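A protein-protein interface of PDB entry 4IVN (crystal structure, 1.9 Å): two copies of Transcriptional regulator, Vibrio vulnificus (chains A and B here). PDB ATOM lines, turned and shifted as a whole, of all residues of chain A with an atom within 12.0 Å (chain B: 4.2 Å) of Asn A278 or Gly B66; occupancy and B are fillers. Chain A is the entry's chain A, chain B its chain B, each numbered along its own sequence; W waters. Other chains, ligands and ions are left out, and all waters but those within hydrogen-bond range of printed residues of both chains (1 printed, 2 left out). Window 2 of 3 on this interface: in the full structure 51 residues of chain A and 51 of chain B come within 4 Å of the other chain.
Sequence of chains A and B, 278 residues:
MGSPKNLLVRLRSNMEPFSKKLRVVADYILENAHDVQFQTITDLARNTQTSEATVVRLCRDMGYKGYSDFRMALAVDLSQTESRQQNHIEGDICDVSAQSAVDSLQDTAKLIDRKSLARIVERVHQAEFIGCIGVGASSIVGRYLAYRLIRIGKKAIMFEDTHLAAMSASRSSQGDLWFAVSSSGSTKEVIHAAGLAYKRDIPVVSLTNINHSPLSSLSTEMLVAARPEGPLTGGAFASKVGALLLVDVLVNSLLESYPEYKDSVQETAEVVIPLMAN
OD1 of Asn A278 lies within hydrogen-bond range of N of Tyr B67.
OD1 of Asn A278 lies within hydrogen-bond range of N of Ser B68 (2.5 Å).
N of Lys B65 lies within hydrogen-bond range of OD2 of Asp B69, 2.8 Å away.
Ile A273 touches Ser B68 (CD1 to O, 3.7 Å).
Asp B69 touches Ile A273 (N to CG2, 3.6 Å).
Met A276 touches Ser B68.
Ile B41 touches Asn A278.
Asn A278 touches Gly B66 (OD1 to C, 3.5 Å).
Of the printed residues of chain B, Ile A273 touches Ser B68 (3.7 Å) and Asp B69 (3.6 Å).
Pro A274 touches none of the printed residues of chain B.
Printed residues of chain B within 4 Å of Met A276: Ser B68 (3.4 Å).
Of chain B, only Ile B41, Gly B66, Tyr B67 and Ser B68 come within 4 Å of Asn A278.
Ile B41 touches just one residue of chain A: Asn A278.
No residue of chain A comes within 4 Å of Cys B59.
Gly B66 touches one residue of chain A.
Of chain A, only Ile A273, Met A276 and Asn A278 come within 4 Å of Ser B68.
Asp B69 touches one residue of chain A.
No residue of chain A comes within 4 Å of Phe B70.
The nearest printed residue of chain B that does not touch Asn A278 is Asp B69 (4.2 Å).
Hydrophobic or aromatic side chains of chain B within 4 Å of the printed part of chain A: Ile B41 and Tyr B67.
Along chain B the printed residues that touch a printed residue of chain A span positions 41 to 69.
Hydrophobic or aromatic side chains of chain A that line the printed part of chain B: Ile A273 and Met A276.
No position is printed for both chains.
Of the 7 pairs that touch across the chains among the printed residues, none has its exchanged pair printed and touching as well.
Water W1 lies within hydrogen-bond range of N of Ile B41 and OXT of Asn A278.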
ATOM      1  N   ALA A 269     -31.476  13.359  22.648  1.00  0.00           N
ATOM      2  CA  ALA A 269     -30.938  14.360  21.705  1.00  0.00           C
ATOM      3  C   ALA A 269     -29.472  14.628  21.979  1.00  0.00           C
ATOM      4  O   ALA A 269     -28.669  14.824  21.056  1.00  0.00           O
ATOM      5  CB  ALA A 269     -31.721  15.699  21.849  1.00  0.00           C
ATOM      6  N   GLU A 270     -29.124  14.737  23.257  1.00  0.00           N
ATOM      7  CA  GLU A 270     -27.740  14.943  23.652  1.00  0.00           C
ATOM      8  C   GLU A 270     -26.795  13.822  23.328  1.00  0.00           C
ATOM      9  O   GLU A 270     -25.658  14.099  22.845  1.00  0.00           O
ATOM     10  CB  GLU A 270     -27.633  15.276  25.195  1.00  0.00           C
ATOM     11  CG  GLU A 270     -28.113  16.724  25.472  1.00  0.00           C
ATOM     12  CD  GLU A 270     -28.252  16.969  26.969  1.00  0.00           C
ATOM     13  OE1 GLU A 270     -28.155  15.972  27.687  1.00  0.00           O
ATOM     14  OE2 GLU A 270     -28.573  18.079  27.428  1.00  0.00           O
ATOM     15  N   VAL A 271     -27.231  12.581  23.457  1.00  0.00           N
ATOM     16  CA  VAL A 271     -26.238  11.516  23.341  1.00  0.00           C
ATOM     17  C   VAL A 271     -25.877  11.181  21.866  1.00  0.00           C
ATOM     18  O   VAL A 271     -24.908  10.384  21.617  1.00  0.00           O
ATOM     19  CB  VAL A 271     -26.615  10.221  24.129  1.00  0.00           C
ATOM     20  CG1 VAL A 271     -26.758  10.494  25.663  1.00  0.00           C
ATOM     21  CG2 VAL A 271     -27.840   9.506  23.493  1.00  0.00           C
ATOM     22  N   VAL A 272     -26.663  11.701  20.922  1.00  0.00           N
ATOM     23  CA  VAL A 272     -26.319  11.508  19.504  1.00  0.00           C
ATOM     24  C   VAL A 272     -25.474  12.660  18.921  1.00  0.00           C
ATOM     25  O   VAL A 272     -24.985  12.587  17.773  1.00  0.00           O
ATOM     26  CB  VAL A 272     -27.560  11.233  18.632  1.00  0.00           C
ATOM     27  CG1 VAL A 272     -28.175   9.881  19.076  1.00  0.00           C
ATOM     28  CG2 VAL A 272     -28.515  12.458  18.663  1.00  0.00           C
ATOM     29  N   ILE A 273     -25.244  13.706  19.715  1.00  0.00           N
ATOM     30  CA  ILE A 273     -24.353  14.834  19.290  1.00  0.00           C
ATOM     31  C   ILE A 273     -22.988  14.319  18.833  1.00  0.00           C
ATOM     32  O   ILE A 273     -22.480  14.750  17.738  1.00  0.00           O
ATOM     33  CB  ILE A 273     -24.240  15.975  20.354  1.00  0.00           C
ATOM     34  CG1 ILE A 273     -25.598  16.623  20.549  1.00  0.00           C
ATOM     35  CG2 ILE A 273     -23.144  17.019  19.974  1.00  0.00           C
ATOM     36  CD1 ILE A 273     -26.160  17.413  19.324  1.00  0.00           C
ATOM     37  N   PRO A 274     -22.402  13.342  19.551  1.00  0.00           N
ATOM     38  CA  PRO A 274     -21.049  12.953  19.053  1.00  0.00           C
ATOM     39  C   PRO A 274     -21.114  12.123  17.762  1.00  0.00           C
ATOM     40  O   PRO A 274     -20.052  11.759  17.220  1.00  0.00           O
ATOM     41  CB  PRO A 274     -20.494  12.029  20.156  1.00  0.00           C
ATOM     42  CG  PRO A 274     -21.289  12.389  21.370  1.00  0.00           C
ATOM     43  CD  PRO A 274     -22.683  12.741  20.886  1.00  0.00           C
ATOM     44  N   LEU A 275     -22.316  11.898  17.234  1.00  0.00           N
ATOM     45  CA  LEU A 275     -22.458  11.125  15.971  1.00  0.00           C
ATOM     46  C   LEU A 275     -22.706  12.089  14.793  1.00  0.00           C
ATOM     47  O   LEU A 275     -22.967  11.637  13.641  1.00  0.00           O
ATOM     48  CB  LEU A 275     -23.603  10.050  16.088  1.00  0.00           C
ATOM     49  CG  LEU A 275     -23.740   9.282  17.417  1.00  0.00           C
ATOM     50  CD1 LEU A 275     -24.882   8.304  17.317  1.00  0.00           C
ATOM     51  CD2 LEU A 275     -22.412   8.528  17.542  1.00  0.00           C
ATOM     52  N   MET A 276     -22.557  13.396  15.044  1.00  0.00           N
ATOM     53  CA  MET A 276     -22.798  14.405  13.977  1.00  0.00           C
ATOM     54  C   MET A 276     -21.463  14.734  13.364  1.00  0.00           C
ATOM     55  O   MET A 276     -20.466  14.504  13.992  1.00  0.00           O
ATOM     56  CB  MET A 276     -23.488  15.692  14.534  1.00  0.00           C
ATOM     57  CG  MET A 276     -24.817  15.416  15.234  1.00  0.00           C
ATOM     58  SD  MET A 276     -25.953  14.825  13.965  1.00  0.00           S
ATOM     59  CE  MET A 276     -26.778  13.590  15.010  1.00  0.00           C
ATOM     60  N   ALA A 277     -21.425  15.303  12.147  1.00  0.00           N
ATOM     61  CA  ALA A 277     -20.156  15.567  11.484  1.00  0.00           C
ATOM     62  C   ALA A 277     -19.503  16.723  12.208  1.00  0.00           C
ATOM     63  O   ALA A 277     -18.281  16.843  12.234  1.00  0.00           O
ATOM     64  CB  ALA A 277     -20.341  15.942  10.029  1.00  0.00           C
ATOM     65  N   ASN A 278     -20.366  17.507  12.843  1.00  0.00           N
ATOM     66  CA  ASN A 278     -20.276  18.947  12.775  1.00  0.00           C
ATOM     67  C   ASN A 278     -20.511  19.640  11.424  1.00  0.00           C
ATOM     68  O   ASN A 278     -19.651  19.711  10.505  1.00  0.00           O
ATOM     69  CB  ASN A 278     -19.065  19.374  13.531  1.00  0.00           C
ATOM     70  CG  ASN A 278     -19.317  19.173  14.983  1.00  0.00           C
ATOM     71  OD1 ASN A 278     -20.100  19.914  15.543  1.00  0.00           O
ATOM     72  ND2 ASN A 278     -18.821  18.080  15.545  1.00  0.00           N
ATOM     73  OXT ASN A 278     -21.675  20.095  11.296  1.00  0.00           O
ATOM     74  N   ILE B  41     -23.854  23.978  10.355  1.00  0.00           N
ATOM     75  CA  ILE B  41     -22.553  24.710  10.356  1.00  0.00           C
ATOM     76  C   ILE B  41     -22.388  25.441   9.030  1.00  0.00           C
ATOM     77  O   ILE B  41     -21.888  26.556   9.039  1.00  0.00           O
ATOM     78  CB  ILE B  41     -21.355  23.795  10.591  1.00  0.00           C
ATOM     79  CG1 ILE B  41     -20.081  24.608  10.888  1.00  0.00           C
ATOM     80  CG2 ILE B  41     -21.163  22.765   9.448  1.00  0.00           C
ATOM     81  CD1 ILE B  41     -18.971  23.613  11.151  1.00  0.00           C
ATOM     82  N   CYS B  59     -16.597  27.802  18.518  1.00  0.00           N
ATOM     83  CA  CYS B  59     -17.218  26.816  19.394  1.00  0.00           C
ATOM     84  C   CYS B  59     -16.230  26.207  20.367  1.00  0.00           C
ATOM     85  O   CYS B  59     -16.518  26.100  21.573  1.00  0.00           O
ATOM     86  CB  CYS B  59     -17.900  25.749  18.520  1.00  0.00           C
ATOM     87  SG  CYS B  59     -19.324  26.473  17.635  1.00  0.00           S
ATOM     88  N   ARG B  60     -15.066  25.829  19.857  1.00  0.00           N
ATOM     89  CA  ARG B  60     -13.945  25.368  20.683  1.00  0.00           C
ATOM     90  C   ARG B  60     -13.479  26.432  21.731  1.00  0.00           C
ATOM     91  O   ARG B  60     -13.281  26.118  22.907  1.00  0.00           O
ATOM     92  CB  ARG B  60     -12.772  25.050  19.776  1.00  0.00           C
ATOM     93  CG  ARG B  60     -12.405  23.614  19.557  1.00  0.00           C
ATOM     94  CD  ARG B  60     -13.230  22.966  18.492  1.00  0.00           C
ATOM     95  NE  ARG B  60     -12.361  22.304  17.525  1.00  0.00           N
ATOM     96  CZ  ARG B  60     -12.720  21.322  16.681  1.00  0.00           C
ATOM     97  NH1 ARG B  60     -13.953  20.817  16.640  1.00  0.00           N
ATOM     98  NH2 ARG B  60     -11.821  20.833  15.849  1.00  0.00           N
ATOM     99  N   TYR B  64     -16.597  24.135  23.812  1.00  0.00           N
ATOM    100  CA  TYR B  64     -17.366  23.026  23.166  1.00  0.00           C
ATOM    101  C   TYR B  64     -16.497  22.197  22.268  1.00  0.00           C
ATOM    102  O   TYR B  64     -15.390  22.574  21.941  1.00  0.00           O
ATOM    103  CB  TYR B  64     -18.633  23.565  22.437  1.00  0.00           C
ATOM    104  CG  TYR B  64     -19.559  24.225  23.444  1.00  0.00           C
ATOM    105  CD1 TYR B  64     -20.362  23.453  24.284  1.00  0.00           C
ATOM    106  CD2 TYR B  64     -19.572  25.625  23.631  1.00  0.00           C
ATOM    107  CE1 TYR B  64     -21.172  24.038  25.234  1.00  0.00           C
ATOM    108  CE2 TYR B  64     -20.388  26.216  24.597  1.00  0.00           C
ATOM    109  CZ  TYR B  64     -21.187  25.421  25.375  1.00  0.00           C
ATOM    110  OH  TYR B  64     -22.009  25.921  26.344  1.00  0.00           O
ATOM    111  N   LYS B  65     -16.974  21.039  21.869  1.00  0.00           N
ATOM    112  CA  LYS B  65     -16.161  20.168  21.038  1.00  0.00           C
ATOM    113  C   LYS B  65     -16.206  20.592  19.582  1.00  0.00           C
ATOM    114  O   LYS B  65     -15.353  20.211  18.782  1.00  0.00           O
ATOM    115  CB  LYS B  65     -16.642  18.717  21.142  1.00  0.00           C
ATOM    116  CG  LYS B  65     -15.695  17.810  21.902  1.00  0.00           C
ATOM    117  CD  LYS B  65     -16.056  17.754  23.363  1.00  0.00           C
ATOM    118  CE  LYS B  65     -15.534  16.450  23.974  1.00  0.00           C
ATOM    119  NZ  LYS B  65     -16.679  15.764  24.589  1.00  0.00           N
ATOM    120  N   GLY B  66     -17.228  21.350  19.211  1.00  0.00           N
ATOM    121  CA  GLY B  66     -17.455  21.626  17.795  1.00  0.00           C
ATOM    122  C   GLY B  66     -18.819  22.288  17.707  1.00  0.00           C
ATOM    123  O   GLY B  66     -19.440  22.652  18.745  1.00  0.00           O
ATOM    124  N   TYR B  67     -19.296  22.449  16.473  1.00  0.00           N
ATOM    125  CA  TYR B  67     -20.523  23.187  16.238  1.00  0.00           C
ATOM    126  C   TYR B  67     -21.803  22.486  16.775  1.00  0.00           C
ATOM    127  O   TYR B  67     -22.604  23.148  17.403  1.00  0.00           O
ATOM    128  CB  TYR B  67     -20.710  23.507  14.768  1.00  0.00           C
ATOM    129  CG  TYR B  67     -22.025  24.215  14.521  1.00  0.00           C
ATOM    130  CD1 TYR B  67     -22.239  25.491  15.028  1.00  0.00           C
ATOM    131  CD2 TYR B  67     -23.090  23.574  13.863  1.00  0.00           C
ATOM    132  CE1 TYR B  67     -23.469  26.139  14.839  1.00  0.00           C
ATOM    133  CE2 TYR B  67     -24.325  24.217  13.690  1.00  0.00           C
ATOM    134  CZ  TYR B  67     -24.489  25.537  14.160  1.00  0.00           C
ATOM    135  OH  TYR B  67     -25.706  26.191  14.028  1.00  0.00           O
ATOM    136  N   SER B  68     -21.988  21.186  16.482  1.00  0.00           N
ATOM    137  CA  SER B  68     -23.107  20.399  16.980  1.00  0.00           C
ATOM    138  C   SER B  68     -23.260  20.466  18.504  1.00  0.00           C
ATOM    139  O   SER B  68     -24.365  20.617  19.010  1.00  0.00           O
ATOM    140  CB  SER B  68     -22.997  18.940  16.451  1.00  0.00           C
ATOM    141  OG  SER B  68     -23.200  18.996  15.026  1.00  0.00           O
ATOM    142  N   ASP B  69     -22.147  20.360  19.213  1.00  0.00           N
ATOM    143  CA  ASP B  69     -22.125  20.407  20.677  1.00  0.00           C
ATOM    144  C   ASP B  69     -22.586  21.791  21.173  1.00  0.00           C
ATOM    145  O   ASP B  69     -23.518  21.898  22.003  1.00  0.00           O
ATOM    146  CB  ASP B  69     -20.695  20.120  21.096  1.00  0.00           C
ATOM    147  CG  ASP B  69     -20.531  19.991  22.596  1.00  0.00           C
ATOM    148  OD1 ASP B  69     -21.493  19.627  23.296  1.00  0.00           O
ATOM    149  OD2 ASP B  69     -19.426  20.257  23.064  1.00  0.00           O
ATOM    150  N   PHE B  70     -21.921  22.843  20.670  1.00  0.00           N
ATOM    151  CA  PHE B  70     -22.359  24.230  20.939  1.00  0.00           C
ATOM    152  C   PHE B  70     -23.874  24.440  20.654  1.00  0.00           C
ATOM    153  O   PHE B  70     -24.585  25.023  21.500  1.00  0.00           O
ATOM    154  CB  PHE B  70     -21.530  25.241  20.084  1.00  0.00           C
ATOM    155  CG  PHE B  70     -22.030  26.649  20.187  1.00  0.00           C
ATOM    156  CD1 PHE B  70     -22.884  27.166  19.235  1.00  0.00           C
ATOM    157  CD2 PHE B  70     -21.601  27.452  21.228  1.00  0.00           C
ATOM    158  CE1 PHE B  70     -23.365  28.467  19.361  1.00  0.00           C
ATOM    159  CE2 PHE B  70     -22.043  28.774  21.348  1.00  0.00           C
ATOM    160  CZ  PHE B  70     -22.936  29.271  20.409  1.00  0.00           C
HETATM  161  O   HOH W   1     -24.347  21.166  10.736  1.00  0.00           O
